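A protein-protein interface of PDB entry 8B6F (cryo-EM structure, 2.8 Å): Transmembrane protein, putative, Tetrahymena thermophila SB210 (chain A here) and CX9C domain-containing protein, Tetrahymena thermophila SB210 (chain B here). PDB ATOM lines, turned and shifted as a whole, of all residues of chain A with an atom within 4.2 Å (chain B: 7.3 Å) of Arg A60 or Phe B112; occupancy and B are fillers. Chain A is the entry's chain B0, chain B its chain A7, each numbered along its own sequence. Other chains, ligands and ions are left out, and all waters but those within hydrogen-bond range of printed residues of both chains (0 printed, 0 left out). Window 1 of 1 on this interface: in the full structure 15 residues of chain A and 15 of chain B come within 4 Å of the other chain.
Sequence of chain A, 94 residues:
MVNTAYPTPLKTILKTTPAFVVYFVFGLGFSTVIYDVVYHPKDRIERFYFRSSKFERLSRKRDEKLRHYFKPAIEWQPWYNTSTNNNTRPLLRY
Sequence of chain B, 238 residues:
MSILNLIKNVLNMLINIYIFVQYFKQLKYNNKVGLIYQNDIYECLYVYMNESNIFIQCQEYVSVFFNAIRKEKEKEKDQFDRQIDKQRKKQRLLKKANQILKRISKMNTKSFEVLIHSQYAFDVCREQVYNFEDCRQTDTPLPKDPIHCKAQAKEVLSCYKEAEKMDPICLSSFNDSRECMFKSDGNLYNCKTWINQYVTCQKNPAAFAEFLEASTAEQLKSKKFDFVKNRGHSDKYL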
ATOM      1  N   ARG A  47     -16.265  -6.161  24.709  1.00  0.00           N
ATOM      2  CA  ARG A  47     -16.053  -6.803  23.422  1.00  0.00           C
ATOM      3  C   ARG A  47     -15.328  -5.856  22.476  1.00  0.00           C
ATOM      4  O   ARG A  47     -15.500  -4.636  22.527  1.00  0.00           O
ATOM      5  CB  ARG A  47     -17.387  -7.240  22.815  1.00  0.00           C
ATOM      6  CG  ARG A  47     -18.199  -8.148  23.723  1.00  0.00           C
ATOM      7  CD  ARG A  47     -19.353  -8.813  22.986  1.00  0.00           C
ATOM      8  NE  ARG A  47     -20.338  -7.852  22.502  1.00  0.00           N
ATOM      9  CZ  ARG A  47     -20.344  -7.318  21.288  1.00  0.00           C
ATOM     10  NH1 ARG A  47     -19.415  -7.618  20.395  1.00  0.00           N
ATOM     11  NH2 ARG A  47     -21.304  -6.461  20.961  1.00  0.00           N
ATOM     12  N   PHE A  48     -14.501  -6.430  21.606  1.00  0.00           N
ATOM     13  CA  PHE A  48     -13.780  -5.620  20.637  1.00  0.00           C
ATOM     14  C   PHE A  48     -14.762  -4.844  19.771  1.00  0.00           C
ATOM     15  O   PHE A  48     -15.862  -5.309  19.463  1.00  0.00           O
ATOM     16  CB  PHE A  48     -12.887  -6.492  19.752  1.00  0.00           C
ATOM     17  CG  PHE A  48     -11.685  -7.066  20.455  1.00  0.00           C
ATOM     18  CD1 PHE A  48     -11.183  -6.486  21.609  1.00  0.00           C
ATOM     19  CD2 PHE A  48     -11.052  -8.186  19.947  1.00  0.00           C
ATOM     20  CE1 PHE A  48     -10.077  -7.014  22.240  1.00  0.00           C
ATOM     21  CE2 PHE A  48      -9.946  -8.718  20.574  1.00  0.00           C
ATOM     22  CZ  PHE A  48      -9.459  -8.133  21.722  1.00  0.00           C
ATOM     23  N   TYR A  49     -14.349  -3.639  19.382  1.00  0.00           N
ATOM     24  CA  TYR A  49     -15.222  -2.782  18.590  1.00  0.00           C
ATOM     25  C   TYR A  49     -15.586  -3.436  17.265  1.00  0.00           C
ATOM     26  O   TYR A  49     -16.748  -3.403  16.847  1.00  0.00           O
ATOM     27  CB  TYR A  49     -14.541  -1.435  18.359  1.00  0.00           C
ATOM     28  CG  TYR A  49     -15.348  -0.484  17.519  1.00  0.00           C
ATOM     29  CD1 TYR A  49     -16.412   0.213  18.063  1.00  0.00           C
ATOM     30  CD2 TYR A  49     -15.034  -0.271  16.187  1.00  0.00           C
ATOM     31  CE1 TYR A  49     -17.149   1.087  17.306  1.00  0.00           C
ATOM     32  CE2 TYR A  49     -15.764   0.602  15.420  1.00  0.00           C
ATOM     33  CZ  TYR A  49     -16.819   1.279  15.986  1.00  0.00           C
ATOM     34  OH  TYR A  49     -17.549   2.147  15.220  1.00  0.00           O
ATOM     35  N   SER A  52     -18.649  -6.430  16.292  1.00  0.00           N
ATOM     36  CA  SER A  52     -19.966  -5.881  16.577  1.00  0.00           C
ATOM     37  C   SER A  52     -20.600  -5.419  15.274  1.00  0.00           C
ATOM     38  O   SER A  52     -19.908  -5.105  14.303  1.00  0.00           O
ATOM     39  CB  SER A  52     -19.870  -4.725  17.579  1.00  0.00           C
ATOM     40  OG  SER A  52     -21.142  -4.386  18.099  1.00  0.00           O
ATOM     41  N   GLU A  56     -24.734  -1.658  16.380  1.00  0.00           N
ATOM     42  CA  GLU A  56     -24.166  -1.753  17.720  1.00  0.00           C
ATOM     43  C   GLU A  56     -22.985  -0.807  17.882  1.00  0.00           C
ATOM     44  O   GLU A  56     -22.845  -0.149  18.920  1.00  0.00           O
ATOM     45  CB  GLU A  56     -23.744  -3.192  18.014  1.00  0.00           C
ATOM     46  CG  GLU A  56     -24.909  -4.155  18.171  1.00  0.00           C
ATOM     47  CD  GLU A  56     -24.461  -5.550  18.558  1.00  0.00           C
ATOM     48  OE1 GLU A  56     -23.323  -5.694  19.048  1.00  0.00           O
ATOM     49  OE2 GLU A  56     -25.245  -6.503  18.367  1.00  0.00           O
ATOM     50  N   ARG A  57     -22.128  -0.719  16.865  1.00  0.00           N
ATOM     51  CA  ARG A  57     -21.005   0.210  16.925  1.00  0.00           C
ATOM     52  C   ARG A  57     -21.496   1.643  17.064  1.00  0.00           C
ATOM     53  O   ARG A  57     -20.977   2.414  17.880  1.00  0.00           O
ATOM     54  CB  ARG A  57     -20.145   0.066  15.671  1.00  0.00           C
ATOM     55  CG  ARG A  57     -19.443  -1.272  15.537  1.00  0.00           C
ATOM     56  CD  ARG A  57     -18.996  -1.498  14.104  1.00  0.00           C
ATOM     57  NE  ARG A  57     -18.386  -2.806  13.914  1.00  0.00           N
ATOM     58  CZ  ARG A  57     -18.010  -3.292  12.740  1.00  0.00           C
ATOM     59  NH1 ARG A  57     -18.176  -2.604  11.623  1.00  0.00           N
ATOM     60  NH2 ARG A  57     -17.454  -4.499  12.683  1.00  0.00           N
ATOM     61  N   LEU A  58     -22.498   2.020  16.270  1.00  0.00           N
ATOM     62  CA  LEU A  58     -23.032   3.374  16.348  1.00  0.00           C
ATOM     63  C   LEU A  58     -23.602   3.663  17.732  1.00  0.00           C
ATOM     64  O   LEU A  58     -23.355   4.731  18.302  1.00  0.00           O
ATOM     65  CB  LEU A  58     -24.099   3.569  15.272  1.00  0.00           C
ATOM     66  CG  LEU A  58     -23.610   4.100  13.922  1.00  0.00           C
ATOM     67  CD1 LEU A  58     -22.306   3.440  13.490  1.00  0.00           C
ATOM     68  CD2 LEU A  58     -24.677   3.896  12.862  1.00  0.00           C
ATOM     69  N   SER A  59     -24.366   2.721  18.288  1.00  0.00           N
ATOM     70  CA  SER A  59     -24.952   2.930  19.608  1.00  0.00           C
ATOM     71  C   SER A  59     -23.874   3.033  20.678  1.00  0.00           C
ATOM     72  O   SER A  59     -23.992   3.834  21.612  1.00  0.00           O
ATOM     73  CB  SER A  59     -25.927   1.800  19.937  1.00  0.00           C
ATOM     74  OG  SER A  59     -25.259   0.553  20.007  1.00  0.00           O
ATOM     75  N   ARG A  60     -22.823   2.220  20.569  1.00  0.00           N
ATOM     76  CA  ARG A  60     -21.749   2.267  21.557  1.00  0.00           C
ATOM     77  C   ARG A  60     -21.009   3.598  21.521  1.00  0.00           C
ATOM     78  O   ARG A  60     -20.694   4.165  22.573  1.00  0.00           O
ATOM     79  CB  ARG A  60     -20.775   1.112  21.316  1.00  0.00           C
ATOM     80  CG  ARG A  60     -21.362  -0.259  21.605  1.00  0.00           C
ATOM     81  CD  ARG A  60     -20.509  -1.374  21.018  1.00  0.00           C
ATOM     82  NE  ARG A  60     -19.246  -1.541  21.728  1.00  0.00           N
ATOM     83  CZ  ARG A  60     -18.329  -2.446  21.419  1.00  0.00           C
ATOM     84  NH1 ARG A  60     -18.494  -3.283  20.408  1.00  0.00           N
ATOM     85  NH2 ARG A  60     -17.215  -2.513  22.142  1.00  0.00           N
ATOM     86  N   LYS A  61     -20.722   4.114  20.327  1.00  0.00           N
ATOM     87  CA  LYS A  61     -19.902   5.310  20.187  1.00  0.00           C
ATOM     88  C   LYS A  61     -20.705   6.603  20.169  1.00  0.00           C
ATOM     89  O   LYS A  61     -20.104   7.680  20.153  1.00  0.00           O
ATOM     90  CB  LYS A  61     -19.062   5.221  18.910  1.00  0.00           C
ATOM     91  CG  LYS A  61     -18.122   4.026  18.873  1.00  0.00           C
ATOM     92  CD  LYS A  61     -17.075   4.102  19.976  1.00  0.00           C
ATOM     93  CE  LYS A  61     -16.214   2.852  20.002  1.00  0.00           C
ATOM     94  NZ  LYS A  61     -15.169   2.922  21.058  1.00  0.00           N
ATOM     95  N   ARG A  62     -22.038   6.531  20.169  1.00  0.00           N
ATOM     96  CA  ARG A  62     -22.840   7.750  20.162  1.00  0.00           C
ATOM     97  C   ARG A  62     -22.537   8.616  21.379  1.00  0.00           C
ATOM     98  O   ARG A  62     -22.330   9.828  21.259  1.00  0.00           O
ATOM     99  CB  ARG A  62     -24.326   7.394  20.112  1.00  0.00           C
ATOM    100  CG  ARG A  62     -25.249   8.595  19.983  1.00  0.00           C
ATOM    101  CD  ARG A  62     -26.704   8.170  20.056  1.00  0.00           C
ATOM    102  NE  ARG A  62     -27.141   7.915  21.425  1.00  0.00           N
ATOM    103  CZ  ARG A  62     -27.779   8.788  22.192  1.00  0.00           C
ATOM    104  NH1 ARG A  62     -28.086  10.000  21.758  1.00  0.00           N
ATOM    105  NH2 ARG A  62     -28.124   8.436  23.426  1.00  0.00           N
ATOM    106  N   THR B 109     -30.030  10.971  28.191  1.00  0.00           N
ATOM    107  CA  THR B 109     -30.063   9.542  28.457  1.00  0.00           C
ATOM    108  C   THR B 109     -28.971   8.853  27.653  1.00  0.00           C
ATOM    109  O   THR B 109     -28.653   9.259  26.532  1.00  0.00           O
ATOM    110  CB  THR B 109     -31.430   8.937  28.096  1.00  0.00           C
ATOM    111  OG1 THR B 109     -32.472   9.673  28.749  1.00  0.00           O
ATOM    112  CG2 THR B 109     -31.506   7.478  28.521  1.00  0.00           C
ATOM    113  N   LYS B 110     -28.393   7.809  28.237  1.00  0.00           N
ATOM    114  CA  LYS B 110     -27.306   7.098  27.588  1.00  0.00           C
ATOM    115  C   LYS B 110     -27.847   6.143  26.524  1.00  0.00           C
ATOM    116  O   LYS B 110     -29.036   5.823  26.477  1.00  0.00           O
ATOM    117  CB  LYS B 110     -26.470   6.350  28.620  1.00  0.00           C
ATOM    118  CG  LYS B 110     -25.922   7.244  29.719  1.00  0.00           C
ATOM    119  CD  LYS B 110     -25.007   6.480  30.657  1.00  0.00           C
ATOM    120  CE  LYS B 110     -24.310   7.418  31.628  1.00  0.00           C
ATOM    121  NZ  LYS B 110     -23.372   6.691  32.527  1.00  0.00           N
ATOM    122  N   SER B 111     -26.939   5.673  25.668  1.00  0.00           N
ATOM    123  CA  SER B 111     -27.347   4.986  24.446  1.00  0.00           C
ATOM    124  C   SER B 111     -28.094   3.692  24.745  1.00  0.00           C
ATOM    125  O   SER B 111     -29.183   3.456  24.213  1.00  0.00           O
ATOM    126  CB  SER B 111     -26.120   4.703  23.582  1.00  0.00           C
ATOM    127  OG  SER B 111     -26.494   4.071  22.371  1.00  0.00           O
ATOM    128  N   PHE B 112     -27.522   2.834  25.592  1.00  0.00           N
ATOM    129  CA  PHE B 112     -28.131   1.530  25.832  1.00  0.00           C
ATOM    130  C   PHE B 112     -29.486   1.672  26.516  1.00  0.00           C
ATOM    131  O   PHE B 112     -30.427   0.939  26.194  1.00  0.00           O
ATOM    132  CB  PHE B 112     -27.190   0.643  26.651  1.00  0.00           C
ATOM    133  CG  PHE B 112     -25.899   0.301  25.941  1.00  0.00           C
ATOM    134  CD1 PHE B 112     -25.710   0.619  24.605  1.00  0.00           C
ATOM    135  CD2 PHE B 112     -24.883  -0.359  26.612  1.00  0.00           C
ATOM    136  CE1 PHE B 112     -24.529   0.298  23.963  1.00  0.00           C
ATOM    137  CE2 PHE B 112     -23.704  -0.681  25.976  1.00  0.00           C
ATOM    138  CZ  PHE B 112     -23.526  -0.353  24.651  1.00  0.00           C
ATOM    139  N   GLU B 113     -29.608   2.609  27.456  1.00  0.00           N
ATOM    140  CA  GLU B 113     -30.909   2.874  28.064  1.00  0.00           C
ATOM    141  C   GLU B 113     -31.905   3.372  27.025  1.00  0.00           C
ATOM    142  O   GLU B 113     -33.092   3.034  27.079  1.00  0.00           O
ATOM    143  CB  GLU B 113     -30.763   3.886  29.198  1.00  0.00           C
ATOM    144  CG  GLU B 113     -29.868   3.410  30.325  1.00  0.00           C
ATOM    145  CD  GLU B 113     -29.746   4.428  31.434  1.00  0.00           C
ATOM    146  OE1 GLU B 113     -30.377   5.499  31.324  1.00  0.00           O
ATOM    147  OE2 GLU B 113     -29.021   4.161  32.413  1.00  0.00           O
ATOM    148  N   VAL B 114     -31.440   4.178  26.069  1.00  0.00           N
ATOM    149  CA  VAL B 114     -32.317   4.636  24.994  1.00  0.00           C
ATOM    150  C   VAL B 114     -32.810   3.451  24.177  1.00  0.00           C
ATOM    151  O   VAL B 114     -33.987   3.381  23.805  1.00  0.00           O
ATOM    152  CB  VAL B 114     -31.594   5.677  24.118  1.00  0.00           C
ATOM    153  CG1 VAL B 114     -32.341   5.905  22.809  1.00  0.00           C
ATOM    154  CG2 VAL B 114     -31.458   6.991  24.866  1.00  0.00           C
ATOM    155  N   LEU B 115     -31.919   2.506  23.873  1.00  0.00           N
ATOM    156  CA  LEU B 115     -32.332   1.314  23.139  1.00  0.00           C
ATOM    157  C   LEU B 115     -33.372   0.525  23.923  1.00  0.00           C
ATOM    158  O   LEU B 115     -34.384   0.085  23.367  1.00  0.00           O
ATOM    159  CB  LEU B 115     -31.118   0.435  22.839  1.00  0.00           C
ATOM    160  CG  LEU B 115     -30.040   1.017  21.926  1.00  0.00           C
ATOM    161  CD1 LEU B 115     -28.801   0.142  21.937  1.00  0.00           C
ATOM    162  CD2 LEU B 115     -30.564   1.175  20.516  1.00  0.00           C
ATOM    163  N   ILE B 116     -33.139   0.334  25.222  1.00  0.00           N
ATOM    164  CA  ILE B 116     -34.071  -0.437  26.041  1.00  0.00           C
ATOM    165  C   ILE B 116     -35.440   0.231  26.049  1.00  0.00           C
ATOM    166  O   ILE B 116     -36.474  -0.426  25.885  1.00  0.00           O
ATOM    167  CB  ILE B 116     -33.515  -0.607  27.466  1.00  0.00           C
ATOM    168  CG1 ILE B 116     -32.229  -1.433  27.435  1.00  0.00           C
ATOM    169  CG2 ILE B 116     -34.544  -1.271  28.373  1.00  0.00           C
ATOM    170  CD1 ILE B 116     -31.447  -1.395  28.726  1.00  0.00           C
ATOM    171  N   HIS B 117     -35.464   1.552  26.234  1.00  0.00           N
ATOM    172  CA  HIS B 117     -36.731   2.276  26.238  1.00  0.00           C
ATOM    173  C   HIS B 117     -37.406   2.215  24.875  1.00  0.00           C
ATOM    174  O   HIS B 117     -38.630   2.065  24.786  1.00  0.00           O
ATOM    175  CB  HIS B 117     -36.505   3.727  26.658  1.00  0.00           C
ATOM    176  CG  HIS B 117     -36.396   3.916  28.137  1.00  0.00           C
ATOM    177  ND1 HIS B 117     -35.398   4.667  28.721  1.00  0.00           N
ATOM    178  CD2 HIS B 117     -37.167   3.462  29.153  1.00  0.00           C
ATOM    179  CE1 HIS B 117     -35.556   4.661  30.032  1.00  0.00           C
ATOM    180  NE2 HIS B 117     -36.622   3.937  30.321  1.00  0.00           N
ATOM    181  N   SER B 118     -36.624   2.320  23.800  1.00  0.00           N
ATOM    182  CA  SER B 118     -37.207   2.272  22.465  1.00  0.00           C
ATOM    183  C   SER B 118     -37.858   0.927  22.185  1.00  0.00           C
ATOM    184  O   SER B 118     -38.878   0.866  21.490  1.00  0.00           O
ATOM    185  CB  SER B 118     -36.133   2.559  21.416  1.00  0.00           C
ATOM    186  OG  SER B 118     -35.567   3.844  21.600  1.00  0.00           O
ATOM    187  N   TYR B 160     -41.524   9.904  22.659  1.00  0.00           N
ATOM    188  CA  TYR B 160     -40.541   9.098  23.369  1.00  0.00           C
ATOM    189  C   TYR B 160     -40.341   9.619  24.786  1.00  0.00           C
ATOM    190  O   TYR B 160     -40.213   8.831  25.730  1.00  0.00           O
ATOM    191  CB  TYR B 160     -39.223   9.088  22.597  1.00  0.00           C
ATOM    192  CG  TYR B 160     -38.138   8.287  23.264  1.00  0.00           C
ATOM    193  CD1 TYR B 160     -38.105   6.902  23.163  1.00  0.00           C
ATOM    194  CD2 TYR B 160     -37.140   8.914  23.991  1.00  0.00           C
ATOM    195  CE1 TYR B 160     -37.112   6.168  23.772  1.00  0.00           C
ATOM    196  CE2 TYR B 160     -36.143   8.188  24.602  1.00  0.00           C
ATOM    197  CZ  TYR B 160     -36.135   6.818  24.490  1.00  0.00           C
ATOM    198  OH  TYR B 160     -35.139   6.100  25.103  1.00  0.00           O
ATOM    199  N   PHE B 174     -35.878  -3.144  34.644  1.00  0.00           N
ATOM    200  CA  PHE B 174     -35.062  -2.171  33.929  1.00  0.00           C
ATOM    201  C   PHE B 174     -33.607  -2.247  34.373  1.00  0.00           C
ATOM    202  O   PHE B 174     -32.692  -2.175  33.545  1.00  0.00           O
ATOM    203  CB  PHE B 174     -35.620  -0.763  34.144  1.00  0.00           C
ATOM    204  CG  PHE B 174     -34.992   0.280  33.263  1.00  0.00           C
ATOM    205  CD1 PHE B 174     -35.059   0.172  31.884  1.00  0.00           C
ATOM    206  CD2 PHE B 174     -34.351   1.376  33.814  1.00  0.00           C
ATOM    207  CE1 PHE B 174     -34.490   1.133  31.070  1.00  0.00           C
ATOM    208  CE2 PHE B 174     -33.781   2.340  33.006  1.00  0.00           C
ATOM    209  CZ  PHE B 174     -33.851   2.218  31.632  1.00  0.00           C
ATOM    210  N   SER B 177     -31.951  -5.424  32.967  1.00  0.00           N
ATOM    211  CA  SER B 177     -31.704  -5.213  31.546  1.00  0.00           C
ATOM    212  C   SER B 177     -30.516  -4.283  31.335  1.00  0.00           C
ATOM    213  O   SER B 177     -29.698  -4.501  30.434  1.00  0.00           O
ATOM    214  CB  SER B 177     -32.957  -4.648  30.879  1.00  0.00           C
ATOM    215  OG  SER B 177     -32.754  -4.470  29.490  1.00  0.00           O
ATOM    216  N   ARG B 178     -30.413  -3.229  32.149  1.00  0.00           N
ATOM    217  CA  ARG B 178     -29.268  -2.330  32.054  1.00  0.00           C
ATOM    218  C   ARG B 178     -27.968  -3.060  32.365  1.00  0.00           C
ATOM    219  O   ARG B 178     -26.959  -2.869  31.679  1.00  0.00           O
ATOM    220  CB  ARG B 178     -29.452  -1.141  32.996  1.00  0.00           C
ATOM    221  CG  ARG B 178     -30.431  -0.099  32.489  1.00  0.00           C
ATOM    222  CD  ARG B 178     -30.680   0.994  33.516  1.00  0.00           C
ATOM    223  NE  ARG B 178     -29.449   1.626  33.978  1.00  0.00           N
ATOM    224  CZ  ARG B 178     -28.779   1.272  35.066  1.00  0.00           C
ATOM    225  NH1 ARG B 178     -29.180   0.271  35.834  1.00  0.00           N
ATOM    226  NH2 ARG B 178     -27.677   1.938  35.395  1.00  0.00           N
ATOM    227  N   CYS B 180     -27.375  -6.259  31.981  1.00  0.00           N
ATOM    228  CA  CYS B 180     -27.084  -7.147  30.862  1.00  0.00           C
ATOM    229  C   CYS B 180     -26.490  -6.369  29.697  1.00  0.00           C
ATOM    230  O   CYS B 180     -25.503  -6.795  29.088  1.00  0.00           O
ATOM    231  CB  CYS B 180     -28.355  -7.879  30.434  1.00  0.00           C
ATOM    232  SG  CYS B 180     -28.086  -9.169  29.199  1.00  0.00           S
ATOM    233  N   MET B 181     -27.086  -5.222  29.368  1.00  0.00           N
ATOM    234  CA  MET B 181     -26.600  -4.413  28.258  1.00  0.00           C
ATOM    235  C   MET B 181     -25.278  -3.728  28.574  1.00  0.00           C
ATOM    236  O   MET B 181     -24.605  -3.256  27.653  1.00  0.00           O
ATOM    237  CB  MET B 181     -27.642  -3.362  27.875  1.00  0.00           C
ATOM    238  CG  MET B 181     -28.875  -3.937  27.202  1.00  0.00           C
ATOM    239  SD  MET B 181     -28.533  -4.592  25.557  1.00  0.00           S
ATOM    240  CE  MET B 181     -28.197  -3.087  24.649  1.00  0.00           C
ATOM    241  N   PHE B 182     -24.903  -3.639  29.850  1.00  0.00           N
ATOM    242  CA  PHE B 182     -23.583  -3.128  30.200  1.00  0.00           C
ATOM    243  C   PHE B 182     -22.518  -4.209  30.061  1.00  0.00           C
ATOM    244  O   PHE B 182     -21.454  -3.972  29.479  1.00  0.00           O
ATOM    245  CB  PHE B 182     -23.598  -2.579  31.628  1.00  0.00           C
ATOM    246  CG  PHE B 182     -22.249  -2.146  32.122  1.00  0.00           C
ATOM    247  CD1 PHE B 182     -21.715  -0.930  31.735  1.00  0.00           C
ATOM    248  CD2 PHE B 182     -21.517  -2.954  32.977  1.00  0.00           C
ATOM    249  CE1 PHE B 182     -20.475  -0.527  32.187  1.00  0.00           C
ATOM    250  CE2 PHE B 182     -20.275  -2.556  33.434  1.00  0.00           C
ATOM    251  CZ  PHE B 182     -19.754  -1.342  33.039  1.00  0.00           C
ATOM    252  N   LYS B 183     -22.788  -5.402  30.591  1.00  0.00           N
ATOM    253  CA  LYS B 183     -21.816  -6.485  30.507  1.00  0.00           C
ATOM    254  C   LYS B 183     -21.600  -6.931  29.066  1.00  0.00           C
ATOM    255  O   LYS B 183     -20.470  -7.242  28.673  1.00  0.00           O
ATOM    256  CB  LYS B 183     -22.270  -7.651  31.383  1.00  0.00           C
ATOM    257  CG  LYS B 183     -22.194  -7.350  32.877  1.00  0.00           C
ATOM    258  CD  LYS B 183     -20.759  -7.136  33.338  1.00  0.00           C
ATOM    259  CE  LYS B 183     -20.686  -6.964  34.845  1.00  0.00           C
ATOM    260  NZ  LYS B 183     -19.279  -6.887  35.321  1.00  0.00           N
ATOM    261  N   SER B 184     -22.660  -6.977  28.266  1.00  0.00           N
ATOM    262  CA  SER B 184     -22.541  -7.189  26.829  1.00  0.00           C
ATOM    263  C   SER B 184     -22.549  -5.832  26.146  1.00  0.00           C
ATOM    264  O   SER B 184     -23.429  -5.007  26.406  1.00  0.00           O
ATOM    265  CB  SER B 184     -23.679  -8.055  26.290  1.00  0.00           C
ATOM    266  OG  SER B 184     -24.943  -7.495  26.601  1.00  0.00           O
ATOM    267  N   ASP B 185     -21.582  -5.606  25.264  1.00  0.00           N
ATOM    268  CA  ASP B 185     -21.410  -4.282  24.687  1.00  0.00           C
ATOM    269  C   ASP B 185     -22.498  -3.983  23.664  1.00  0.00           C
ATOM    270  O   ASP B 185     -22.229  -3.910  22.462  1.00  0.00           O
ATOM    271  CB  ASP B 185     -20.025  -4.160  24.055  1.00  0.00           C
ATOM    272  CG  ASP B 185     -18.912  -4.218  25.082  1.00  0.00           C
ATOM    273  OD1 ASP B 185     -18.594  -5.328  25.558  1.00  0.00           O
ATOM    274  OD2 ASP B 185     -18.359  -3.152  25.421  1.00  0.00           O
ATOM    275  N   GLY B 186     -23.730  -3.807  24.136  1.00  0.00           N
ATOM    276  CA  GLY B 186     -24.814  -3.375  23.280  1.00  0.00           C
ATOM    277  C   GLY B 186     -25.470  -4.458  22.457  1.00  0.00           C
ATOM    278  O   GLY B 186     -26.219  -4.134  21.530  1.00  0.00           O
ATOM    279  N   ASN B 187     -25.220  -5.728  22.755  1.00  0.00           N
ATOM    280  CA  ASN B 187     -25.827  -6.822  22.001  1.00  0.00           C
ATOM    281  C   ASN B 187     -27.268  -6.973  22.469  1.00  0.00           C
ATOM    282  O   ASN B 187     -27.533  -7.496  23.553  1.00  0.00           O
ATOM    283  CB  ASN B 187     -25.037  -8.110  22.188  1.00  0.00           C
ATOM    284  CG  ASN B 187     -25.341  -9.137  21.118  1.00  0.00           C
ATOM    285  OD1 ASN B 187     -26.471  -9.247  20.650  1.00  0.00           O
ATOM    286  ND2 ASN B 187     -24.324  -9.892  20.718  1.00  0.00           N
ATOM    287  N   LEU B 188     -28.211  -6.509  21.645  1.00  0.00           N
ATOM    288  CA  LEU B 188     -29.618  -6.552  22.030  1.00  0.00           C
ATOM    289  C   LEU B 188     -30.140  -7.981  22.082  1.00  0.00           C
ATOM    290  O   LEU B 188     -30.967  -8.313  22.938  1.00  0.00           O
ATOM    291  CB  LEU B 188     -30.450  -5.715  21.059  1.00  0.00           C
ATOM    292  CG  LEU B 188     -30.326  -4.194  21.181  1.00  0.00           C
ATOM    293  CD1 LEU B 188     -30.972  -3.508  19.993  1.00  0.00           C
ATOM    294  CD2 LEU B 188     -30.952  -3.706  22.477  1.00  0.00           C
ATOM    295  N   ILE B 195     -34.993  -7.435  28.322  1.00  0.00           N
ATOM    296  CA  ILE B 195     -35.718  -6.338  27.691  1.00  0.00           C
ATOM    297  C   ILE B 195     -37.170  -6.732  27.460  1.00  0.00           C
ATOM    298  O   ILE B 195     -38.083  -5.916  27.620  1.00  0.00           O
ATOM    299  CB  ILE B 195     -35.029  -5.925  26.377  1.00  0.00           C
ATOM    300  CG1 ILE B 195     -33.615  -5.413  26.660  1.00  0.00           C
ATOM    301  CG2 ILE B 195     -35.852  -4.866  25.653  1.00  0.00           C
ATOM    302  CD1 ILE B 195     -32.786  -5.155  25.419  1.00  0.00           C
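Gly B186 touches Glu A56. Asn B187 touches Glu A56 (CA to OE2, 3.7 Å). Leu B115 touches Ser A59 (CD1 to CB, 3.9 Å). Phe B112 touches Arg A60 (CZ to CG, 3.7 Å). Arg A62 touches Lys B110. CA of Ser B111 touches NH2 of Arg A62, at 3.7 Å. Val B114 touches Arg A62.
Arg A60 touches two residues of chain B. Of chain A, only Arg A60 (3.7 Å) comes within 4 Å of Phe B112. Printed residues of chain B within 4 Å of Ser A59: Ser B111 (2.6 Å) and Leu B115 (3.9 Å). Of the printed residues of chain A, Leu B115 touches Ser A59 (3.9 Å). Printed residues of chain B within 4 Å of Arg A47: Asp B185 (2.6 Å). Of the printed residues of chain A, Asp B185 touches Arg A47 (2.6 Å) and Arg A60 (3.4 Å). Of the printed residues of chain B, Glu A56 touches Gly B186 (3.6 Å) and Asn B187 (3.7 Å). The nearest residue of chain A that does not touch Phe B112 is Ser A59 (4.03 Å).
The side-chain carboxylate (OD1) of Asp B185 sits at hydrogen-bond distance from the backbone NH (N) of Arg A47, at 2.6 Å. O of Ser A59 is in hydrogen-bond range of OG of Ser B111 (2.6 Å). NH2 of Arg A60 is in salt-bridge range of OD2 of Asp B185, 3.5 Å away. The guanidinium group (NH2) of Arg A62 is in hydrogen-bond range of the backbone carbonyl oxygen (O) of Thr B109.
The guanidinium group (NH2) of Arg A47 is in salt-bridge range of the side-chain carboxylate (OE1) of Glu A56 (2.9 Å). O of Arg A47 lies within hydrogen-bond range of NH2 of Arg A60 (2.8 Å). The backbone carbonyl oxygen (O) of Phe A48 lies within hydrogen-bond range of the guanidinium group (NH1) of Arg A60 (3.5 Å). OG of Ser A52 is in hydrogen-bond range of OE1 of Glu A56 (2.7 Å). O of Glu A56 is in hydrogen-bond range of OG of Ser A59 (2.7 Å). The backbone carbonyl oxygen (O) of Val B114 lies within hydrogen-bond range of the side-chain hydroxyl (OG) of Ser B118 (2.8 Å).
Of the 24 printed residues of chain B, 9 touch a printed residue of chain A. Hydrophobic or aromatic side chains of chain B that line the printed part of chain A: Phe B112, Val B114 and Leu B115. Of the 11 printed residues of chain A, 5 touch a printed residue of chain B.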
